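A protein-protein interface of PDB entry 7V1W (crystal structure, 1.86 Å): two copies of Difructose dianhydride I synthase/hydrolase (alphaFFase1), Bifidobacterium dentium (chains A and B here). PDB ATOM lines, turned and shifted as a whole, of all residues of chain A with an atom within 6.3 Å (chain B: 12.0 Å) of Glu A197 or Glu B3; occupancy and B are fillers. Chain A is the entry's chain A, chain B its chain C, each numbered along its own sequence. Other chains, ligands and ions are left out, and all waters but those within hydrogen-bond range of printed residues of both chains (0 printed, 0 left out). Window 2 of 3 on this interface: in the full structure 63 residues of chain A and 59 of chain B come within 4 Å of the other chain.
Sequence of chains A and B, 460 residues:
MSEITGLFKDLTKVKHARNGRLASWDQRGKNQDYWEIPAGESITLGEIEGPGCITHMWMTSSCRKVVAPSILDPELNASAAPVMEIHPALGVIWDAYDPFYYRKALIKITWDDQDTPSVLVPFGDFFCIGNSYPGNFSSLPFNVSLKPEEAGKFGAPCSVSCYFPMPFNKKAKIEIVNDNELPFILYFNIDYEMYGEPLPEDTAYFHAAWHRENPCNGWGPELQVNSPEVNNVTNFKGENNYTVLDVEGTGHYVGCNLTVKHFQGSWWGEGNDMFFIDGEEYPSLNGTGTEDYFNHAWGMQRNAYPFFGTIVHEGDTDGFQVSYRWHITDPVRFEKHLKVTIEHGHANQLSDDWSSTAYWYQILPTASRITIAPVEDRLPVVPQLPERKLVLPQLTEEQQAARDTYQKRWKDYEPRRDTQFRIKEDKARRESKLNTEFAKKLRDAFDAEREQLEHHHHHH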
ATOM      1  N   LYS A  15      30.694 -14.127 -22.410  1.00  0.00           N
ATOM      2  CA  LYS A  15      29.734 -15.199 -22.765  1.00  0.00           C
ATOM      3  C   LYS A  15      28.833 -14.679 -23.868  1.00  0.00           C
ATOM      4  O   LYS A  15      28.328 -13.560 -23.725  1.00  0.00           O
ATOM      5  CB  LYS A  15      28.914 -15.649 -21.561  1.00  0.00           C
ATOM      6  CG  LYS A  15      28.471 -17.096 -21.661  1.00  0.00           C
ATOM      7  CD  LYS A  15      27.300 -17.388 -20.756  1.00  0.00           C
ATOM      8  CE  LYS A  15      27.642 -17.213 -19.293  1.00  0.00           C
ATOM      9  NZ  LYS A  15      26.506 -17.580 -18.413  1.00  0.00           N
ATOM     10  N   HIS A  16      28.669 -15.465 -24.931  1.00  0.00           N
ATOM     11  CA  HIS A  16      27.822 -15.102 -26.093  1.00  0.00           C
ATOM     12  C   HIS A  16      26.389 -15.460 -25.725  1.00  0.00           C
ATOM     13  O   HIS A  16      25.839 -16.431 -26.299  1.00  0.00           O
ATOM     14  CB  HIS A  16      28.391 -15.718 -27.381  1.00  0.00           C
ATOM     15  CG  HIS A  16      29.795 -15.259 -27.626  1.00  0.00           C
ATOM     16  ND1 HIS A  16      30.121 -13.905 -27.705  1.00  0.00           N
ATOM     17  CD2 HIS A  16      30.962 -15.940 -27.735  1.00  0.00           C
ATOM     18  CE1 HIS A  16      31.429 -13.775 -27.894  1.00  0.00           C
ATOM     19  NE2 HIS A  16      31.966 -15.010 -27.898  1.00  0.00           N
ATOM     20  N   PRO A  51      16.878 -22.136 -24.806  1.00  0.00           N
ATOM     21  CA  PRO A  51      17.588 -22.356 -23.553  1.00  0.00           C
ATOM     22  C   PRO A  51      17.927 -21.010 -22.878  1.00  0.00           C
ATOM     23  O   PRO A  51      18.188 -20.014 -23.546  1.00  0.00           O
ATOM     24  CB  PRO A  51      18.849 -23.121 -23.977  1.00  0.00           C
ATOM     25  CG  PRO A  51      18.760 -23.270 -25.502  1.00  0.00           C
ATOM     26  CD  PRO A  51      17.746 -22.260 -25.979  1.00  0.00           C
ATOM     27  N   ASN A 169      15.926 -25.451 -20.344  1.00  0.00           N
ATOM     28  CA  ASN A 169      16.352 -25.788 -21.728  1.00  0.00           C
ATOM     29  C   ASN A 169      15.255 -25.376 -22.695  1.00  0.00           C
ATOM     30  O   ASN A 169      15.619 -24.920 -23.769  1.00  0.00           O
ATOM     31  CB  ASN A 169      16.800 -27.244 -21.891  1.00  0.00           C
ATOM     32  CG  ASN A 169      18.307 -27.333 -22.040  1.00  0.00           C
ATOM     33  OD1 ASN A 169      18.966 -26.345 -22.371  1.00  0.00           O
ATOM     34  ND2 ASN A 169      18.878 -28.500 -21.785  1.00  0.00           N
ATOM     35  N   GLU A 193      19.304 -14.602 -18.987  1.00  0.00           N
ATOM     36  CA  GLU A 193      20.108 -14.626 -20.226  1.00  0.00           C
ATOM     37  C   GLU A 193      19.650 -15.822 -21.073  1.00  0.00           C
ATOM     38  O   GLU A 193      19.124 -16.778 -20.511  1.00  0.00           O
ATOM     39  CB  GLU A 193      21.592 -14.551 -19.878  1.00  0.00           C
ATOM     40  CG  GLU A 193      22.098 -15.665 -19.015  1.00  0.00           C
ATOM     41  CD  GLU A 193      23.545 -15.510 -18.567  1.00  0.00           C
ATOM     42  OE1 GLU A 193      24.024 -14.373 -18.451  1.00  0.00           O
ATOM     43  OE2 GLU A 193      24.183 -16.542 -18.321  1.00  0.00           O
ATOM     44  N   TYR A 195      20.740 -18.610 -24.171  1.00  0.00           N
ATOM     45  CA  TYR A 195      21.939 -19.308 -24.676  1.00  0.00           C
ATOM     46  C   TYR A 195      21.706 -19.685 -26.136  1.00  0.00           C
ATOM     47  O   TYR A 195      20.533 -19.788 -26.538  1.00  0.00           O
ATOM     48  CB  TYR A 195      22.270 -20.491 -23.768  1.00  0.00           C
ATOM     49  CG  TYR A 195      22.447 -20.069 -22.333  1.00  0.00           C
ATOM     50  CD1 TYR A 195      23.269 -18.998 -22.003  1.00  0.00           C
ATOM     51  CD2 TYR A 195      21.765 -20.708 -21.308  1.00  0.00           C
ATOM     52  CE1 TYR A 195      23.435 -18.599 -20.681  1.00  0.00           C
ATOM     53  CE2 TYR A 195      21.905 -20.307 -19.984  1.00  0.00           C
ATOM     54  CZ  TYR A 195      22.735 -19.240 -19.671  1.00  0.00           C
ATOM     55  OH  TYR A 195      22.874 -18.862 -18.370  1.00  0.00           O
ATOM     56  N   GLY A 196      22.802 -19.809 -26.892  1.00  0.00           N
ATOM     57  CA  GLY A 196      22.785 -20.119 -28.337  1.00  0.00           C
ATOM     58  C   GLY A 196      22.818 -21.617 -28.573  1.00  0.00           C
ATOM     59  O   GLY A 196      22.647 -22.009 -29.712  1.00  0.00           O
ATOM     60  N   GLU A 197      23.082 -22.413 -27.533  1.00  0.00           N
ATOM     61  CA  GLU A 197      23.067 -23.899 -27.586  1.00  0.00           C
ATOM     62  C   GLU A 197      22.328 -24.410 -26.357  1.00  0.00           C
ATOM     63  O   GLU A 197      22.229 -23.707 -25.351  1.00  0.00           O
ATOM     64  CB  GLU A 197      24.481 -24.496 -27.644  1.00  0.00           C
ATOM     65  CG  GLU A 197      25.578 -23.511 -28.033  1.00  0.00           C
ATOM     66  CD  GLU A 197      26.214 -22.778 -26.850  1.00  0.00           C
ATOM     67  OE1 GLU A 197      26.153 -21.516 -26.815  1.00  0.00           O
ATOM     68  OE2 GLU A 197      26.769 -23.471 -25.956  1.00  0.00           O
ATOM     69  N   PRO A 198      21.820 -25.660 -26.387  1.00  0.00           N
ATOM     70  CA  PRO A 198      21.194 -26.272 -25.207  1.00  0.00           C
ATOM     71  C   PRO A 198      22.154 -26.399 -24.011  1.00  0.00           C
ATOM     72  O   PRO A 198      23.316 -26.573 -24.229  1.00  0.00           O
ATOM     73  CB  PRO A 198      20.779 -27.663 -25.710  1.00  0.00           C
ATOM     74  CG  PRO A 198      20.653 -27.474 -27.212  1.00  0.00           C
ATOM     75  CD  PRO A 198      21.804 -26.554 -27.555  1.00  0.00           C
ATOM     76  N   LEU A 199      21.636 -26.325 -22.785  1.00  0.00           N
ATOM     77  CA  LEU A 199      22.370 -26.708 -21.550  1.00  0.00           C
ATOM     78  C   LEU A 199      22.538 -28.228 -21.552  1.00  0.00           C
ATOM     79  O   LEU A 199      21.757 -28.922 -22.195  1.00  0.00           O
ATOM     80  CB  LEU A 199      21.573 -26.232 -20.334  1.00  0.00           C
ATOM     81  CG  LEU A 199      21.386 -24.718 -20.245  1.00  0.00           C
ATOM     82  CD1 LEU A 199      20.167 -24.384 -19.423  1.00  0.00           C
ATOM     83  CD2 LEU A 199      22.627 -24.035 -19.691  1.00  0.00           C
ATOM     84  N   PRO A 200      23.527 -28.816 -20.848  1.00  0.00           N
ATOM     85  CA  PRO A 200      23.597 -30.279 -20.747  1.00  0.00           C
ATOM     86  C   PRO A 200      22.245 -30.808 -20.244  1.00  0.00           C
ATOM     87  O   PRO A 200      21.623 -30.119 -19.479  1.00  0.00           O
ATOM     88  CB  PRO A 200      24.752 -30.505 -19.773  1.00  0.00           C
ATOM     89  CG  PRO A 200      25.609 -29.269 -19.920  1.00  0.00           C
ATOM     90  CD  PRO A 200      24.627 -28.138 -20.146  1.00  0.00           C
ATOM     91  N   ARG A 443      14.001 -13.611 -28.294  1.00  0.00           N
ATOM     92  CA  ARG A 443      14.509 -14.993 -28.503  1.00  0.00           C
ATOM     93  C   ARG A 443      14.827 -15.153 -29.994  1.00  0.00           C
ATOM     94  O   ARG A 443      15.943 -15.576 -30.315  1.00  0.00           O
ATOM     95  CB  ARG A 443      13.421 -15.965 -28.044  1.00  0.00           C
ATOM     96  CG  ARG A 443      13.656 -17.417 -28.438  1.00  0.00           C
ATOM     97  CD  ARG A 443      14.518 -18.099 -27.399  1.00  0.00           C
ATOM     98  NE  ARG A 443      15.932 -18.152 -27.707  1.00  0.00           N
ATOM     99  CZ  ARG A 443      16.877 -18.517 -26.847  1.00  0.00           C
ATOM    100  NH1 ARG A 443      16.575 -18.812 -25.597  1.00  0.00           N
ATOM    101  NH2 ARG A 443      18.135 -18.594 -27.238  1.00  0.00           N
ATOM    102  N   PHE A 446      17.725 -12.966 -31.378  1.00  0.00           N
ATOM    103  CA  PHE A 446      19.011 -13.532 -30.891  1.00  0.00           C
ATOM    104  C   PHE A 446      19.380 -14.777 -31.717  1.00  0.00           C
ATOM    105  O   PHE A 446      20.535 -14.870 -32.199  1.00  0.00           O
ATOM    106  CB  PHE A 446      18.922 -13.856 -29.397  1.00  0.00           C
ATOM    107  CG  PHE A 446      20.114 -14.589 -28.839  1.00  0.00           C
ATOM    108  CD1 PHE A 446      21.377 -14.030 -28.895  1.00  0.00           C
ATOM    109  CD2 PHE A 446      19.966 -15.836 -28.250  1.00  0.00           C
ATOM    110  CE1 PHE A 446      22.472 -14.704 -28.377  1.00  0.00           C
ATOM    111  CE2 PHE A 446      21.050 -16.485 -27.681  1.00  0.00           C
ATOM    112  CZ  PHE A 446      22.303 -15.932 -27.763  1.00  0.00           C
ATOM    113  N   GLU B   3      26.668 -21.566 -21.336  1.00  0.00           N
ATOM    114  CA  GLU B   3      26.479 -22.416 -20.106  1.00  0.00           C
ATOM    115  C   GLU B   3      26.502 -21.507 -18.878  1.00  0.00           C
ATOM    116  O   GLU B   3      26.804 -20.297 -19.027  1.00  0.00           O
ATOM    117  CB  GLU B   3      27.513 -23.541 -20.018  1.00  0.00           C
ATOM    118  CG  GLU B   3      27.561 -24.381 -21.289  1.00  0.00           C
ATOM    119  CD  GLU B   3      26.299 -24.373 -22.157  1.00  0.00           C
ATOM    120  OE1 GLU B   3      25.974 -23.326 -22.785  1.00  0.00           O
ATOM    121  OE2 GLU B   3      25.632 -25.416 -22.213  1.00  0.00           O
ATOM    122  N   ILE B   4      26.126 -22.055 -17.724  1.00  0.00           N
ATOM    123  CA  ILE B   4      25.794 -21.245 -16.513  1.00  0.00           C
ATOM    124  C   ILE B   4      27.121 -20.752 -15.908  1.00  0.00           C
ATOM    125  O   ILE B   4      28.041 -21.572 -15.784  1.00  0.00           O
ATOM    126  CB  ILE B   4      24.959 -22.081 -15.515  1.00  0.00           C
ATOM    127  CG1 ILE B   4      23.793 -22.814 -16.181  1.00  0.00           C
ATOM    128  CG2 ILE B   4      24.478 -21.225 -14.358  1.00  0.00           C
ATOM    129  CD1 ILE B   4      22.790 -21.902 -16.849  1.00  0.00           C
ATOM    130  N   THR B   5      27.232 -19.477 -15.543  1.00  0.00           N
ATOM    131  CA  THR B   5      28.456 -18.919 -14.902  1.00  0.00           C
ATOM    132  C   THR B   5      28.114 -18.286 -13.545  1.00  0.00           C
ATOM    133  O   THR B   5      26.913 -18.251 -13.179  1.00  0.00           O
ATOM    134  CB  THR B   5      29.160 -17.915 -15.821  1.00  0.00           C
ATOM    135  OG1 THR B   5      28.189 -16.950 -16.210  1.00  0.00           O
ATOM    136  CG2 THR B   5      29.787 -18.570 -17.033  1.00  0.00           C
ATOM    137  N   GLY B   6      29.152 -17.804 -12.852  1.00  0.00           N
ATOM    138  CA  GLY B   6      29.090 -17.122 -11.547  1.00  0.00           C
ATOM    139  C   GLY B   6      29.148 -18.078 -10.365  1.00  0.00           C
ATOM    140  O   GLY B   6      29.141 -19.322 -10.548  1.00  0.00           O
ATOM    141  N   LEU B   7      29.131 -17.520  -9.156  1.00  0.00           N
ATOM    142  CA  LEU B   7      29.460 -18.261  -7.908  1.00  0.00           C
ATOM    143  C   LEU B   7      28.364 -19.273  -7.540  1.00  0.00           C
ATOM    144  O   LEU B   7      28.677 -20.178  -6.760  1.00  0.00           O
ATOM    145  CB  LEU B   7      29.750 -17.267  -6.771  1.00  0.00           C
ATOM    146  CG  LEU B   7      28.597 -16.383  -6.290  1.00  0.00           C
ATOM    147  CD1 LEU B   7      27.773 -17.088  -5.215  1.00  0.00           C
ATOM    148  CD2 LEU B   7      29.136 -15.055  -5.758  1.00  0.00           C
ATOM    149  N   PHE B   8      27.132 -19.146  -8.042  1.00  0.00           N
ATOM    150  CA  PHE B   8      26.069 -20.155  -7.766  1.00  0.00           C
ATOM    151  C   PHE B   8      26.057 -21.275  -8.811  1.00  0.00           C
ATOM    152  O   PHE B   8      25.156 -22.114  -8.692  1.00  0.00           O
ATOM    153  CB  PHE B   8      24.673 -19.528  -7.717  1.00  0.00           C
ATOM    154  CG  PHE B   8      24.475 -18.448  -6.687  1.00  0.00           C
ATOM    155  CD1 PHE B   8      24.233 -18.764  -5.361  1.00  0.00           C
ATOM    156  CD2 PHE B   8      24.406 -17.116  -7.064  1.00  0.00           C
ATOM    157  CE1 PHE B   8      24.006 -17.763  -4.422  1.00  0.00           C
ATOM    158  CE2 PHE B   8      24.169 -16.119  -6.131  1.00  0.00           C
ATOM    159  CZ  PHE B   8      23.972 -16.447  -4.808  1.00  0.00           C
ATOM    160  N   LYS B   9      26.949 -21.277  -9.816  1.00  0.00           N
ATOM    161  CA  LYS B   9      26.797 -22.142 -11.018  1.00  0.00           C
ATOM    162  C   LYS B   9      26.793 -23.629 -10.624  1.00  0.00           C
ATOM    163  O   LYS B   9      26.039 -24.378 -11.244  1.00  0.00           O
ATOM    164  CB  LYS B   9      27.877 -21.872 -12.073  1.00  0.00           C
ATOM    165  CG  LYS B   9      29.292 -22.290 -11.711  1.00  0.00           C
ATOM    166  CD  LYS B   9      30.256 -22.046 -12.879  1.00  0.00           C
ATOM    167  CE  LYS B   9      31.709 -21.944 -12.475  1.00  0.00           C
ATOM    168  NZ  LYS B   9      32.238 -23.246 -11.994  1.00  0.00           N
ATOM    169  N   ASP B  10      27.549 -24.054  -9.618  1.00  0.00           N
ATOM    170  CA  ASP B  10      27.673 -25.500  -9.288  1.00  0.00           C
ATOM    171  C   ASP B  10      26.341 -26.048  -8.750  1.00  0.00           C
ATOM    172  O   ASP B  10      26.149 -27.276  -8.804  1.00  0.00           O
ATOM    173  CB  ASP B  10      28.830 -25.753  -8.327  1.00  0.00           C
ATOM    174  CG  ASP B  10      30.190 -25.553  -8.976  1.00  0.00           C
ATOM    175  OD1 ASP B  10      30.242 -25.504 -10.221  1.00  0.00           O
ATOM    176  OD2 ASP B  10      31.186 -25.429  -8.238  1.00  0.00           O
ATOM    177  N   LEU B  11      25.413 -25.189  -8.309  1.00  0.00           N
ATOM    178  CA  LEU B  11      24.059 -25.655  -7.894  1.00  0.00           C
ATOM    179  C   LEU B  11      23.269 -26.178  -9.103  1.00  0.00           C
ATOM    180  O   LEU B  11      22.268 -26.855  -8.857  1.00  0.00           O
ATOM    181  CB  LEU B  11      23.281 -24.520  -7.223  1.00  0.00           C
ATOM    182  CG  LEU B  11      23.904 -23.937  -5.956  1.00  0.00           C
ATOM    183  CD1 LEU B  11      23.019 -22.818  -5.433  1.00  0.00           C
ATOM    184  CD2 LEU B  11      24.129 -24.982  -4.898  1.00  0.00           C
ATOM    185  N   THR B  12      23.664 -25.851 -10.339  1.00  0.00           N
ATOM    186  CA  THR B  12      22.909 -26.227 -11.564  1.00  0.00           C
ATOM    187  C   THR B  12      23.423 -27.538 -12.193  1.00  0.00           C
ATOM    188  O   THR B  12      22.963 -27.850 -13.312  1.00  0.00           O
ATOM    189  CB  THR B  12      22.905 -25.104 -12.599  1.00  0.00           C
ATOM    190  OG1 THR B  12      24.234 -24.882 -13.067  1.00  0.00           O
ATOM    191  CG2 THR B  12      22.299 -23.828 -12.061  1.00  0.00           C
ATOM    192  N   LYS B  13      24.309 -28.298 -11.541  1.00  0.00           N
ATOM    193  CA  LYS B  13      24.703 -29.638 -12.050  1.00  0.00           C
ATOM    194  C   LYS B  13      24.789 -30.620 -10.881  1.00  0.00           C
ATOM    195  O   LYS B  13      25.293 -30.249  -9.822  1.00  0.00           O
ATOM    196  CB  LYS B  13      26.005 -29.605 -12.860  1.00  0.00           C
ATOM    197  CG  LYS B  13      27.187 -28.945 -12.178  1.00  0.00           C
ATOM    198  CD  LYS B  13      28.503 -29.661 -12.396  1.00  0.00           C
ATOM    199  CE  LYS B  13      29.579 -29.157 -11.449  1.00  0.00           C
ATOM    200  NZ  LYS B  13      29.767 -27.690 -11.578  1.00  0.00           N
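NZ of Lys A15 is in hydrogen-bond range of O of Glu B3 (2.8 Å). NZ of Lys A15 is in hydrogen-bond range of OG1 of Thr B5. The side-chain carboxylate of Glu A197 lies close to the side-chain carboxylate of Glu B3, at 3.3 Å. OE2 of Glu B3 lies close to O of Pro A198 (3.3 Å).
NZ of Lys A15 lies within salt-bridge range of OE2 of Glu A193 (2.5 Å). O of Pro A51 lies within hydrogen-bond range of N of Tyr A195. OD1 of Asn A169 is in hydrogen-bond range of N of Leu A199 (2.7 Å). The side-chain carboxylate of Glu A193 lies within hydrogen-bond range of the side-chain hydroxyl of Tyr A195, at 2.7 Å. The backbone carbonyl oxygen of Tyr A195 is in hydrogen-bond range of the guanidinium group of Arg A443, 2.8 Å away.
Tyr A195 touches Ile B4 (OH to CD1, 3.4 Å). Glu B3 touches Leu A199. Leu A199 touches Ile B4. Glu B3 touches Pro A200.
Of the printed residues of chain B, Lys A15 touches Glu B3 and Thr B5. Tyr A195 touches one residue of chain B. Pro A198 touches one residue of chain B. Leu A199 touches just these residues of chain B: Glu B3 and Ile B4. Pro A200 touches one residue of chain B. Glu B3 touches just these residues of chain A: Lys A15, Glu A197, Pro A198, Leu A199 and Pro A200. Of the printed residues of chain A, Ile B4 touches Tyr A195 (3.4 Å) and Leu A199 (3.6 Å). Printed residues of chain A within 4 Å of Thr B5: Lys A15 (2.8 Å). Gly B6 touches none of the printed residues of chain A. Thr B12 touches none of the printed residues of chain A. The nearest residue of chain B that does not touch Glu A197 is Ile B4 (8.4 Å).
Printed residues of chain A that touch a printed residue of chain B: Lys A15, Tyr A195, Glu A197, Pro A198, Leu A199 and Pro A200. Hydrophobic or aromatic side chains of chain B within 4 Å of the printed part of chain A: Ile B4. Among the printed residues, no Asp or Glu carboxylate lies within 4 Å of a Lys or Arg side-chain nitrogen of the other chain.
No position is printed for both chains. Of the 8 pairs that touch across the chains among the printed residues, none has its exchanged pair printed and touching as well.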
